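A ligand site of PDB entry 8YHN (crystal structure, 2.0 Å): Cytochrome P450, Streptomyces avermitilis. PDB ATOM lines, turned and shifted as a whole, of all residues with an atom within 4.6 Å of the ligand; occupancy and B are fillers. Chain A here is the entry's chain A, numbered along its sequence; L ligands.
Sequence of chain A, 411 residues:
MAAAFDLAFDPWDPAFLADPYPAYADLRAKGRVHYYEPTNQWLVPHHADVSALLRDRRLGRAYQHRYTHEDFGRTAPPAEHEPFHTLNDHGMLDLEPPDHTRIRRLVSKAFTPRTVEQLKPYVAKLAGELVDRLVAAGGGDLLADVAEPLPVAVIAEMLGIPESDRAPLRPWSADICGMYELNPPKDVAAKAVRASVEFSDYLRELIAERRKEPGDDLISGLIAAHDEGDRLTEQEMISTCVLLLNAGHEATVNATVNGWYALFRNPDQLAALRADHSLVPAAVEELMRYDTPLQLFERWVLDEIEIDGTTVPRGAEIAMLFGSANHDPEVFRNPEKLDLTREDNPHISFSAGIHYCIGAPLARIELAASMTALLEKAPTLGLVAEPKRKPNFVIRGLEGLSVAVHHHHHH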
ATOM      1  N   LEU A  54     -11.643 -20.069   3.470  1.00  0.00           N
ATOM      2  CA  LEU A  54     -11.655 -18.635   3.913  1.00  0.00           C
ATOM      3  C   LEU A  54     -12.856 -17.883   3.322  1.00  0.00           C
ATOM      4  O   LEU A  54     -13.230 -16.813   3.868  1.00  0.00           O
ATOM      5  CB  LEU A  54     -10.352 -17.968   3.485  1.00  0.00           C
ATOM      6  CG  LEU A  54      -9.091 -18.372   4.246  1.00  0.00           C
ATOM      7  CD1 LEU A  54      -7.850 -17.879   3.505  1.00  0.00           C
ATOM      8  CD2 LEU A  54      -9.132 -17.832   5.658  1.00  0.00           C
ATOM      9  N   ARG A  61     -14.433 -16.894  12.385  1.00  0.00           N
ATOM     10  CA  ARG A  61     -13.472 -16.649  13.488  1.00  0.00           C
ATOM     11  C   ARG A  61     -14.232 -16.531  14.808  1.00  0.00           C
ATOM     12  O   ARG A  61     -13.565 -16.420  15.850  1.00  0.00           O
ATOM     13  CB  ARG A  61     -12.648 -15.395  13.165  1.00  0.00           C
ATOM     14  CG  ARG A  61     -11.588 -15.658  12.107  1.00  0.00           C
ATOM     15  CD  ARG A  61     -10.695 -14.458  11.956  1.00  0.00           C
ATOM     16  NE  ARG A  61     -10.064 -14.237  13.238  1.00  0.00           N
ATOM     17  CZ  ARG A  61      -8.836 -14.621  13.569  1.00  0.00           C
ATOM     18  NH1 ARG A  61      -8.399 -14.351  14.788  1.00  0.00           N
ATOM     19  NH2 ARG A  61      -8.007 -15.177  12.687  1.00  0.00           N
ATOM     20  N   MET A  92     -12.938  -6.078  14.492  1.00  0.00           N
ATOM     21  CA  MET A  92     -13.541  -6.758  13.324  1.00  0.00           C
ATOM     22  C   MET A  92     -12.869  -8.113  13.026  1.00  0.00           C
ATOM     23  O   MET A  92     -13.533  -8.960  12.415  1.00  0.00           O
ATOM     24  CB  MET A  92     -13.530  -5.840  12.099  1.00  0.00           C
ATOM     25  CG  MET A  92     -12.189  -5.672  11.421  1.00  0.00           C
ATOM     26  SD  MET A  92     -12.296  -4.352  10.172  1.00  0.00           S
ATOM     27  CE  MET A  92     -12.333  -2.918  11.232  1.00  0.00           C
ATOM     28  N   LEU A  93     -11.623  -8.365  13.458  1.00  0.00           N
ATOM     29  CA  LEU A  93     -10.935  -9.662  13.216  1.00  0.00           C
ATOM     30  C   LEU A  93     -11.748 -10.825  13.790  1.00  0.00           C
ATOM     31  O   LEU A  93     -11.764 -11.889  13.166  1.00  0.00           O
ATOM     32  CB  LEU A  93      -9.538  -9.647  13.855  1.00  0.00           C
ATOM     33  CG  LEU A  93      -8.395 -10.386  13.158  1.00  0.00           C
ATOM     34  CD1 LEU A  93      -7.568 -11.136  14.184  1.00  0.00           C
ATOM     35  CD2 LEU A  93      -8.802 -11.300  12.002  1.00  0.00           C
ATOM     36  N   HIS A 100     -19.628  -7.806  11.551  1.00  0.00           N
ATOM     37  CA  HIS A 100     -18.349  -7.598  10.818  1.00  0.00           C
ATOM     38  C   HIS A 100     -18.556  -6.551   9.705  1.00  0.00           C
ATOM     39  O   HIS A 100     -17.803  -5.522   9.674  1.00  0.00           O
ATOM     40  CB  HIS A 100     -17.787  -8.910  10.227  1.00  0.00           C
ATOM     41  CG  HIS A 100     -16.546  -8.682   9.422  1.00  0.00           C
ATOM     42  ND1 HIS A 100     -16.588  -8.559   8.040  1.00  0.00           N
ATOM     43  CD2 HIS A 100     -15.246  -8.517   9.790  1.00  0.00           C
ATOM     44  CE1 HIS A 100     -15.362  -8.320   7.592  1.00  0.00           C
ATOM     45  NE2 HIS A 100     -14.522  -8.295   8.642  1.00  0.00           N
ATOM     46  N   ARG A 104     -16.779  -2.887   9.565  1.00  0.00           N
ATOM     47  CA  ARG A 104     -15.774  -2.766   8.477  1.00  0.00           C
ATOM     48  C   ARG A 104     -16.231  -1.671   7.496  1.00  0.00           C
ATOM     49  O   ARG A 104     -15.385  -0.839   7.111  1.00  0.00           O
ATOM     50  CB  ARG A 104     -15.479  -4.100   7.768  1.00  0.00           C
ATOM     51  CG  ARG A 104     -14.398  -3.984   6.704  1.00  0.00           C
ATOM     52  CD  ARG A 104     -13.573  -5.243   6.490  1.00  0.00           C
ATOM     53  NE  ARG A 104     -12.547  -5.094   5.456  1.00  0.00           N
ATOM     54  CZ  ARG A 104     -11.564  -5.955   5.209  1.00  0.00           C
ATOM     55  NH1 ARG A 104     -11.414  -7.067   5.921  1.00  0.00           N
ATOM     56  NH2 ARG A 104     -10.731  -5.707   4.215  1.00  0.00           N
ATOM     57  N   ILE A 155       1.431   3.500  12.407  1.00  0.00           N
ATOM     58  CA  ILE A 155       0.046   3.370  12.929  1.00  0.00           C
ATOM     59  C   ILE A 155      -0.183   4.476  13.960  1.00  0.00           C
ATOM     60  O   ILE A 155      -1.205   5.158  13.849  1.00  0.00           O
ATOM     61  CB  ILE A 155      -0.234   1.950  13.458  1.00  0.00           C
ATOM     62  CG1 ILE A 155      -0.096   0.915  12.345  1.00  0.00           C
ATOM     63  CG2 ILE A 155      -1.605   1.864  14.108  1.00  0.00           C
ATOM     64  CD1 ILE A 155       0.254  -0.458  12.845  1.00  0.00           C
ATOM     65  N   LEU A 243      -6.641  -3.001  17.488  1.00  0.00           N
ATOM     66  CA  LEU A 243      -6.532  -4.020  16.412  1.00  0.00           C
ATOM     67  C   LEU A 243      -5.536  -3.485  15.369  1.00  0.00           C
ATOM     68  O   LEU A 243      -4.589  -4.203  15.048  1.00  0.00           O
ATOM     69  CB  LEU A 243      -7.911  -4.266  15.783  1.00  0.00           C
ATOM     70  CG  LEU A 243      -7.959  -5.255  14.610  1.00  0.00           C
ATOM     71  CD1 LEU A 243      -7.320  -6.586  14.973  1.00  0.00           C
ATOM     72  CD2 LEU A 243      -9.383  -5.453  14.134  1.00  0.00           C
ATOM     73  N   LEU A 244      -5.707  -2.242  14.935  1.00  0.00           N
ATOM     74  CA  LEU A 244      -4.831  -1.670  13.892  1.00  0.00           C
ATOM     75  C   LEU A 244      -3.373  -1.743  14.366  1.00  0.00           C
ATOM     76  O   LEU A 244      -2.514  -2.203  13.594  1.00  0.00           O
ATOM     77  CB  LEU A 244      -5.299  -0.251  13.543  1.00  0.00           C
ATOM     78  CG  LEU A 244      -6.647  -0.184  12.827  1.00  0.00           C
ATOM     79  CD1 LEU A 244      -7.135   1.242  12.706  1.00  0.00           C
ATOM     80  CD2 LEU A 244      -6.596  -0.836  11.453  1.00  0.00           C
ATOM     81  N   ALA A 247      -2.436  -5.748  14.725  1.00  0.00           N
ATOM     82  CA  ALA A 247      -2.441  -6.412  13.395  1.00  0.00           C
ATOM     83  C   ALA A 247      -1.305  -5.888  12.521  1.00  0.00           C
ATOM     84  O   ALA A 247      -0.711  -6.672  11.793  1.00  0.00           O
ATOM     85  CB  ALA A 247      -3.799  -6.234  12.747  1.00  0.00           C
ATOM     86  N   GLY A 248      -1.021  -4.579  12.579  1.00  0.00           N
ATOM     87  CA  GLY A 248      -0.066  -3.916  11.692  1.00  0.00           C
ATOM     88  C   GLY A 248       1.361  -3.922  12.210  1.00  0.00           C
ATOM     89  O   GLY A 248       2.237  -3.366  11.493  1.00  0.00           O
ATOM     90  N   ALA A 251       3.445  -8.633  12.217  1.00  0.00           N
ATOM     91  CA  ALA A 251       3.387  -9.223  10.862  1.00  0.00           C
ATOM     92  C   ALA A 251       4.363  -8.441   9.980  1.00  0.00           C
ATOM     93  O   ALA A 251       5.211  -9.051   9.296  1.00  0.00           O
ATOM     94  CB  ALA A 251       1.978  -9.197  10.332  1.00  0.00           C
ATOM     95  N   THR A 252       4.271  -7.115   9.998  1.00  0.00           N
ATOM     96  CA  THR A 252       5.093  -6.242   9.125  1.00  0.00           C
ATOM     97  C   THR A 252       6.564  -6.414   9.524  1.00  0.00           C
ATOM     98  O   THR A 252       7.432  -6.561   8.625  1.00  0.00           O
ATOM     99  CB  THR A 252       4.552  -4.809   9.159  1.00  0.00           C
ATOM    100  OG1 THR A 252       3.134  -4.846   8.997  1.00  0.00           O
ATOM    101  CG2 THR A 252       5.184  -3.934   8.099  1.00  0.00           C
ATOM    102  N   ALA A 255       7.884  -9.872   8.321  1.00  0.00           N
ATOM    103  CA  ALA A 255       7.986  -9.912   6.840  1.00  0.00           C
ATOM    104  C   ALA A 255       9.293  -9.251   6.391  1.00  0.00           C
ATOM    105  O   ALA A 255       9.969  -9.771   5.478  1.00  0.00           O
ATOM    106  CB  ALA A 255       6.809  -9.251   6.178  1.00  0.00           C
ATOM    107  N   MET A 288       7.284 -12.646   0.736  1.00  0.00           N
ATOM    108  CA  MET A 288       6.129 -13.046   1.572  1.00  0.00           C
ATOM    109  C   MET A 288       5.672 -14.478   1.217  1.00  0.00           C
ATOM    110  O   MET A 288       5.582 -15.332   2.130  1.00  0.00           O
ATOM    111  CB  MET A 288       4.971 -12.071   1.423  1.00  0.00           C
ATOM    112  CG  MET A 288       4.068 -12.114   2.619  1.00  0.00           C
ATOM    113  SD  MET A 288       2.925 -10.720   2.628  1.00  0.00           S
ATOM    114  CE  MET A 288       4.068  -9.338   2.532  1.00  0.00           C
ATOM    115  N   LEU A 294       3.033 -15.169   8.910  1.00  0.00           N
ATOM    116  CA  LEU A 294       1.745 -15.706   9.449  1.00  0.00           C
ATOM    117  C   LEU A 294       1.451 -17.057   8.798  1.00  0.00           C
ATOM    118  O   LEU A 294       0.794 -17.092   7.728  1.00  0.00           O
ATOM    119  CB  LEU A 294       0.622 -14.693   9.244  1.00  0.00           C
ATOM    120  CG  LEU A 294       0.915 -13.313   9.805  1.00  0.00           C
ATOM    121  CD1 LEU A 294      -0.175 -12.301   9.482  1.00  0.00           C
ATOM    122  CD2 LEU A 294       1.149 -13.372  11.299  1.00  0.00           C
ATOM    123  N   PHE A 297      -3.896 -19.942  10.444  1.00  0.00           N
ATOM    124  CA  PHE A 297      -5.151 -19.258  10.822  1.00  0.00           C
ATOM    125  C   PHE A 297      -6.191 -20.335  11.021  1.00  0.00           C
ATOM    126  O   PHE A 297      -6.159 -21.369  10.321  1.00  0.00           O
ATOM    127  CB  PHE A 297      -5.529 -18.187   9.808  1.00  0.00           C
ATOM    128  CG  PHE A 297      -4.655 -16.977   9.918  1.00  0.00           C
ATOM    129  CD1 PHE A 297      -4.849 -16.047  10.932  1.00  0.00           C
ATOM    130  CD2 PHE A 297      -3.545 -16.842   9.099  1.00  0.00           C
ATOM    131  CE1 PHE A 297      -3.993 -14.977  11.087  1.00  0.00           C
ATOM    132  CE2 PHE A 297      -2.704 -15.757   9.241  1.00  0.00           C
ATOM    133  CZ  PHE A 297      -2.934 -14.829  10.233  1.00  0.00           C
ATOM    134  N   ARG A 299     -10.437 -21.467  11.844  1.00  0.00           N
ATOM    135  CA  ARG A 299     -11.877 -21.181  11.675  1.00  0.00           C
ATOM    136  C   ARG A 299     -12.646 -22.239  12.461  1.00  0.00           C
ATOM    137  O   ARG A 299     -12.270 -23.406  12.440  1.00  0.00           O
ATOM    138  CB  ARG A 299     -12.252 -21.196  10.178  1.00  0.00           C
ATOM    139  CG  ARG A 299     -11.690 -20.026   9.378  1.00  0.00           C
ATOM    140  CD  ARG A 299     -12.280 -18.710   9.812  1.00  0.00           C
ATOM    141  NE  ARG A 299     -11.972 -17.621   8.920  1.00  0.00           N
ATOM    142  CZ  ARG A 299     -10.825 -16.945   8.901  1.00  0.00           C
ATOM    143  NH1 ARG A 299      -9.837 -17.262   9.719  1.00  0.00           N
ATOM    144  NH2 ARG A 299     -10.675 -15.949   8.061  1.00  0.00           N
ATOM    145  N   PHE A 322      -1.176 -21.542   5.846  1.00  0.00           N
ATOM    146  CA  PHE A 322      -0.871 -20.507   4.817  1.00  0.00           C
ATOM    147  C   PHE A 322       0.521 -20.794   4.218  1.00  0.00           C
ATOM    148  O   PHE A 322       0.690 -20.622   3.016  1.00  0.00           O
ATOM    149  CB  PHE A 322      -0.942 -19.097   5.418  1.00  0.00           C
ATOM    150  CG  PHE A 322      -2.325 -18.510   5.549  1.00  0.00           C
ATOM    151  CD1 PHE A 322      -3.436 -19.315   5.770  1.00  0.00           C
ATOM    152  CD2 PHE A 322      -2.509 -17.136   5.440  1.00  0.00           C
ATOM    153  CE1 PHE A 322      -4.701 -18.767   5.869  1.00  0.00           C
ATOM    154  CE2 PHE A 322      -3.777 -16.590   5.548  1.00  0.00           C
ATOM    155  CZ  PHE A 322      -4.873 -17.399   5.784  1.00  0.00           C
ATOM    156  N   SER A 349      -1.110 -14.695   1.462  1.00  0.00           N
ATOM    157  CA  SER A 349      -0.484 -14.288   2.742  1.00  0.00           C
ATOM    158  C   SER A 349      -1.396 -13.271   3.440  1.00  0.00           C
ATOM    159  O   SER A 349      -1.345 -13.189   4.667  1.00  0.00           O
ATOM    160  CB  SER A 349       0.916 -13.727   2.570  1.00  0.00           C
ATOM    161  OG  SER A 349       1.814 -14.660   1.977  1.00  0.00           O
ATOM    162  N   PHE A 350      -2.240 -12.534   2.693  1.00  0.00           N
ATOM    163  CA  PHE A 350      -3.156 -11.519   3.252  1.00  0.00           C
ATOM    164  C   PHE A 350      -4.555 -12.116   3.397  1.00  0.00           C
ATOM    165  O   PHE A 350      -5.486 -11.329   3.670  1.00  0.00           O
ATOM    166  CB  PHE A 350      -3.178 -10.218   2.440  1.00  0.00           C
ATOM    167  CG  PHE A 350      -1.895  -9.439   2.533  1.00  0.00           C
ATOM    168  CD1 PHE A 350      -1.627  -8.662   3.644  1.00  0.00           C
ATOM    169  CD2 PHE A 350      -0.964  -9.496   1.510  1.00  0.00           C
ATOM    170  CE1 PHE A 350      -0.436  -7.955   3.750  1.00  0.00           C
ATOM    171  CE2 PHE A 350       0.217  -8.763   1.595  1.00  0.00           C
ATOM    172  CZ  PHE A 350       0.489  -8.009   2.715  1.00  0.00           C
ATOM    173  N   SER A 351      -4.673 -13.451   3.258  1.00  0.00           N
ATOM    174  CA  SER A 351      -5.908 -14.221   3.490  1.00  0.00           C
ATOM    175  C   SER A 351      -6.921 -13.939   2.361  1.00  0.00           C
ATOM    176  O   SER A 351      -6.520 -13.453   1.336  1.00  0.00           O
ATOM    177  CB  SER A 351      -6.508 -13.874   4.844  1.00  0.00           C
ATOM    178  OG  SER A 351      -7.503 -14.823   5.194  1.00  0.00           O
ATOM    179  N   ILE A 354     -14.076 -12.523   4.019  1.00  0.00           N
ATOM    180  CA  ILE A 354     -14.453 -11.247   4.715  1.00  0.00           C
ATOM    181  C   ILE A 354     -13.291 -10.734   5.585  1.00  0.00           C
ATOM    182  O   ILE A 354     -13.205  -9.531   5.787  1.00  0.00           O
ATOM    183  CB  ILE A 354     -15.760 -11.427   5.529  1.00  0.00           C
ATOM    184  CG1 ILE A 354     -15.576 -12.418   6.686  1.00  0.00           C
ATOM    185  CG2 ILE A 354     -16.907 -11.853   4.625  1.00  0.00           C
ATOM    186  CD1 ILE A 354     -16.779 -12.491   7.613  1.00  0.00           C
ATOM    187  N   HIS A 355     -12.381 -11.607   6.044  1.00  0.00           N
ATOM    188  CA  HIS A 355     -11.281 -11.196   6.952  1.00  0.00           C
ATOM    189  C   HIS A 355     -10.030 -10.759   6.174  1.00  0.00           C
ATOM    190  O   HIS A 355      -8.991 -10.494   6.827  1.00  0.00           O
ATOM    191  CB  HIS A 355     -11.053 -12.302   7.988  1.00  0.00           C
ATOM    192  CG  HIS A 355     -12.202 -12.439   8.943  1.00  0.00           C
ATOM    193  ND1 HIS A 355     -12.549 -11.428   9.806  1.00  0.00           N
ATOM    194  CD2 HIS A 355     -13.074 -13.454   9.184  1.00  0.00           C
ATOM    195  CE1 HIS A 355     -13.558 -11.832  10.570  1.00  0.00           C
ATOM    196  NE2 HIS A 355     -13.932 -13.051  10.180  1.00  0.00           N
ATOM    197  N   TYR A 356     -10.088 -10.757   4.841  1.00  0.00           N
ATOM    198  CA  TYR A 356      -8.980 -10.280   3.961  1.00  0.00           C
ATOM    199  C   TYR A 356      -8.433  -8.979   4.545  1.00  0.00           C
ATOM    200  O   TYR A 356      -9.231  -8.086   4.867  1.00  0.00           O
ATOM    201  CB  TYR A 356      -9.453 -10.058   2.524  1.00  0.00           C
ATOM    202  CG  TYR A 356      -8.425  -9.404   1.637  1.00  0.00           C
ATOM    203  CD1 TYR A 356      -7.332 -10.106   1.142  1.00  0.00           C
ATOM    204  CD2 TYR A 356      -8.561  -8.072   1.250  1.00  0.00           C
ATOM    205  CE1 TYR A 356      -6.408  -9.507   0.288  1.00  0.00           C
ATOM    206  CE2 TYR A 356      -7.645  -7.453   0.397  1.00  0.00           C
ATOM    207  CZ  TYR A 356      -6.558  -8.167  -0.081  1.00  0.00           C
ATOM    208  OH  TYR A 356      -5.665  -7.537  -0.918  1.00  0.00           O
ATOM    209  N   CYS A 357      -7.116  -8.943   4.728  1.00  0.00           N
ATOM    210  CA  CYS A 357      -6.398  -7.893   5.474  1.00  0.00           C
ATOM    211  C   CYS A 357      -6.763  -6.517   4.917  1.00  0.00           C
ATOM    212  O   CYS A 357      -6.406  -6.217   3.773  1.00  0.00           O
ATOM    213  CB  CYS A 357      -4.898  -8.116   5.396  1.00  0.00           C
ATOM    214  SG  CYS A 357      -3.965  -6.869   6.294  1.00  0.00           S
ATOM    215  N   ILE A 358      -7.439  -5.699   5.731  1.00  0.00           N
ATOM    216  CA  ILE A 358      -7.756  -4.296   5.363  1.00  0.00           C
ATOM    217  C   ILE A 358      -6.460  -3.461   5.331  1.00  0.00           C
ATOM    218  O   ILE A 358      -6.442  -2.417   4.691  1.00  0.00           O
ATOM    219  CB  ILE A 358      -8.792  -3.724   6.353  1.00  0.00           C
ATOM    220  CG1 ILE A 358      -9.390  -2.416   5.829  1.00  0.00           C
ATOM    221  CG2 ILE A 358      -8.195  -3.540   7.735  1.00  0.00           C
ATOM    222  CD1 ILE A 358     -10.391  -1.794   6.805  1.00  0.00           C
ATOM    223  N   GLY A 359      -5.407  -3.924   6.008  1.00  0.00           N
ATOM    224  CA  GLY A 359      -4.107  -3.232   6.017  1.00  0.00           C
ATOM    225  C   GLY A 359      -3.192  -3.511   4.826  1.00  0.00           C
ATOM    226  O   GLY A 359      -2.120  -2.912   4.834  1.00  0.00           O
ATOM    227  N   LEU A 362      -1.336  -0.695   2.896  1.00  0.00           N
ATOM    228  CA  LEU A 362      -0.394   0.053   3.768  1.00  0.00           C
ATOM    229  C   LEU A 362       0.816  -0.840   4.084  1.00  0.00           C
ATOM    230  O   LEU A 362       1.939  -0.321   4.042  1.00  0.00           O
ATOM    231  CB  LEU A 362      -1.092   0.543   5.041  1.00  0.00           C
ATOM    232  CG  LEU A 362      -0.211   1.256   6.068  1.00  0.00           C
ATOM    233  CD1 LEU A 362       0.586   2.385   5.420  1.00  0.00           C
ATOM    234  CD2 LEU A 362      -1.030   1.818   7.219  1.00  0.00           C
ATOM    235  N   ALA A 363       0.586  -2.107   4.388  1.00  0.00           N
ATOM    236  CA  ALA A 363       1.656  -3.103   4.644  1.00  0.00           C
ATOM    237  C   ALA A 363       2.625  -3.100   3.452  1.00  0.00           C
ATOM    238  O   ALA A 363       3.834  -2.964   3.671  1.00  0.00           O
ATOM    239  CB  ALA A 363       1.061  -4.449   4.917  1.00  0.00           C
ATOM    240  N   GLU A 366       4.760   0.016   3.397  1.00  0.00           N
ATOM    241  CA  GLU A 366       5.835   0.025   4.423  1.00  0.00           C
ATOM    242  C   GLU A 366       6.969  -0.938   4.025  1.00  0.00           C
ATOM    243  O   GLU A 366       8.164  -0.586   4.254  1.00  0.00           O
ATOM    244  CB  GLU A 366       5.322  -0.364   5.800  1.00  0.00           C
ATOM    245  CG  GLU A 366       4.138   0.470   6.256  1.00  0.00           C
ATOM    246  CD  GLU A 366       3.662   0.092   7.658  1.00  0.00           C
ATOM    247  OE1 GLU A 366       2.465   0.328   7.980  1.00  0.00           O
ATOM    248  OE2 GLU A 366       4.491  -0.429   8.414  1.00  0.00           O
ATOM    249  N   LEU A 367       6.628  -2.108   3.473  1.00  0.00           N
ATOM    250  CA  LEU A 367       7.661  -3.131   3.130  1.00  0.00           C
ATOM    251  C   LEU A 367       8.509  -2.613   1.963  1.00  0.00           C
ATOM    252  O   LEU A 367       9.719  -2.807   2.033  1.00  0.00           O
ATOM    253  CB  LEU A 367       6.998  -4.473   2.820  1.00  0.00           C
ATOM    254  CG  LEU A 367       6.304  -5.122   4.025  1.00  0.00           C
ATOM    255  CD1 LEU A 367       5.441  -6.291   3.607  1.00  0.00           C
ATOM    256  CD2 LEU A 367       7.331  -5.573   5.066  1.00  0.00           C
HETATM  257  C1  LIG L   1      -6.369  -9.252   8.929  1.00  0.00           C
HETATM  258  C2  LIG L   1      -2.082 -10.565   7.103  1.00  0.00           C
HETATM  259  C3  LIG L   1      -0.366  -6.163   7.977  1.00  0.00           C
HETATM  260  C4  LIG L   1      -4.675  -4.867   9.644  1.00  0.00           C
HETATM  261  C5  LIG L   1      -5.340 -10.013   8.362  1.00  0.00           C
HETATM  262  C6  LIG L   1      -5.429 -11.362   8.071  1.00  0.00           C
HETATM  263  C7  LIG L   1      -4.218 -11.728   7.573  1.00  0.00           C
HETATM  264  C8  LIG L   1      -3.393 -10.595   7.538  1.00  0.00           C
HETATM  265  C9  LIG L   1      -3.825 -13.101   7.089  1.00  0.00           C
HETATM  266  C10 LIG L   1      -6.629 -12.267   8.238  1.00  0.00           C
HETATM  267  C11 LIG L   1      -6.454 -13.442   9.193  1.00  0.00           C
HETATM  268  C12 LIG L   1      -7.577 -14.477   9.034  1.00  0.00           C
HETATM  269  O1  LIG L   1      -7.986 -15.245   9.936  1.00  0.00           O
HETATM  270  O2  LIG L   1      -8.161 -14.624   7.969  1.00  0.00           O
HETATM  271  C13 LIG L   1      -1.222  -9.467   7.222  1.00  0.00           C
HETATM  272  C14 LIG L   1       0.150  -9.530   6.845  1.00  0.00           C
HETATM  273  C15 LIG L   1       0.627  -8.272   7.083  1.00  0.00           C
HETATM  274  C16 LIG L   1      -0.500  -7.495   7.632  1.00  0.00           C
HETATM  275  C17 LIG L   1       0.909 -10.710   6.242  1.00  0.00           C
HETATM  276  C18 LIG L   1       1.944  -7.664   6.935  1.00  0.00           C
HETATM  277  C19 LIG L   1       3.022  -8.325   6.602  1.00  0.00           C
HETATM  278  C20 LIG L   1      -1.367  -5.379   8.461  1.00  0.00           C
HETATM  279  C21 LIG L   1      -1.336  -4.007   8.673  1.00  0.00           C
HETATM  280  C22 LIG L   1      -2.594  -3.683   9.161  1.00  0.00           C
HETATM  281  C23 LIG L   1      -3.366  -4.847   9.207  1.00  0.00           C
HETATM  282  C24 LIG L   1      -0.132  -3.067   8.439  1.00  0.00           C
HETATM  283  C25 LIG L   1      -3.192  -2.397   9.598  1.00  0.00           C
HETATM  284  C26 LIG L   1      -2.598  -1.248   9.536  1.00  0.00           C
HETATM  285  C27 LIG L   1      -5.454  -5.980   9.601  1.00  0.00           C
HETATM  286  C28 LIG L   1      -6.848  -5.909  10.100  1.00  0.00           C
HETATM  287  C29 LIG L   1      -7.327  -7.156   9.916  1.00  0.00           C
HETATM  288  C30 LIG L   1      -6.202  -7.938   9.291  1.00  0.00           C
HETATM  289  C31 LIG L   1      -7.519  -4.707  10.744  1.00  0.00           C
HETATM  290  C32 LIG L   1      -8.704  -7.709  10.234  1.00  0.00           C
HETATM  291  C33 LIG L   1      -9.575  -7.667   8.930  1.00  0.00           C
HETATM  292  C34 LIG L   1     -10.972  -8.215   9.137  1.00  0.00           C
HETATM  293  O3  LIG L   1     -11.938  -7.795   8.459  1.00  0.00           O
HETATM  294  O4  LIG L   1     -11.163  -9.090  10.016  1.00  0.00           O
HETATM  295  N1  LIG L   1      -4.085  -9.537   8.047  1.00  0.00           N
HETATM  296  N2  LIG L   1      -1.537  -8.268   7.649  1.00  0.00           N
HETATM  297  N3  LIG L   1      -2.604  -5.852   8.750  1.00  0.00           N
HETATM  298  N4  LIG L   1      -5.140  -7.160   9.081  1.00  0.00           N
HETATM  299 FE1  LIG L   1      -3.440  -7.665   8.289  1.00  0.00          FE
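A ring nitrogen (NE2) of His 100 lies within hydrogen-bond range of an oxygen (O3) of the ligand (2.6 Å). ND1 of His 355 is in hydrogen-bond range of O4 of the ligand. NH2 of Arg 61 is in salt-bridge range of O1 of the ligand. An oxygen (O3) of the ligand lies within salt-bridge range of the guanidinium group (NH1) of Arg 104 (2.7 Å). The side-chain sulfur of Cys 357 is bound to an iron atom (FE1) of the ligand, 2.2 Å away. An oxygen (O2) of the ligand sits at hydrogen-bond distance from the side-chain hydroxyl of Ser 351, 2.9 Å away. An oxygen (O1) of the ligand is in salt-bridge range of the guanidinium group (NH1) of Arg 299 (2.7 Å).
The backbone NH (N) of Cys 357 is in hydrogen-bond range of the backbone carbonyl oxygen (O) of Phe 350 (3.1 Å). O of Leu 93 is in hydrogen-bond range of NE of Arg 61, 2.9 Å away. The backbone carbonyl oxygen (O) of Ile 354 lies within hydrogen-bond range of the guanidinium group (NH1) of Arg 104. The backbone carbonyl oxygen of Gly 248 sits at hydrogen-bond distance from the side-chain hydroxyl of Thr 252, 3.0 Å away. A ring nitrogen (NE2) of His 100 lies close to the backbone carbonyl oxygen (O) of Ile 354, at 3.4 Å. The guanidinium group (NH1) of Arg 104 is in hydrogen-bond range of the backbone carbonyl oxygen (O) of Tyr 356 (2.6 Å). The side-chain sulfur of Cys 357 sits close to the backbone NH of Gly 359, 3.3 Å away. The backbone carbonyl oxygen of Leu 93 lies close to a ring nitrogen (ND1) of His 355 (3.5 Å).
O4 of the ligand sits close to O of Met 92 (3.4 Å). O of Ile 354 sits close to O3 of the ligand (3.4 Å). Residues that only touch the ligand: Leu 93 (3.3 Å), Leu 243 (3.9 Å), Ala 247 (3.5 Å), Gly 248 (3.3 Å), Ala 251 (3.5 Å), Thr 252 (3.7 Å), Ala 255 (3.9 Å), Leu 294 (3.5 Å), Phe 297 (3.4 Å), Phe 322 (3.8 Å), Ser 349 (3.5 Å), Phe 350 (3.5 Å), Ile 358 (3.3 Å), Gly 359 (3.5 Å) and Ala 363 (3.8 Å). Hydrophobic or aromatic side chains within 4 Å of the ligand: Met 92, Leu 93, His 100, Leu 243, Ala 247, Ala 251, Ala 255, Leu 294, Phe 297, Phe 322, Phe 350, His 355, Ile 358 and Ala 363.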
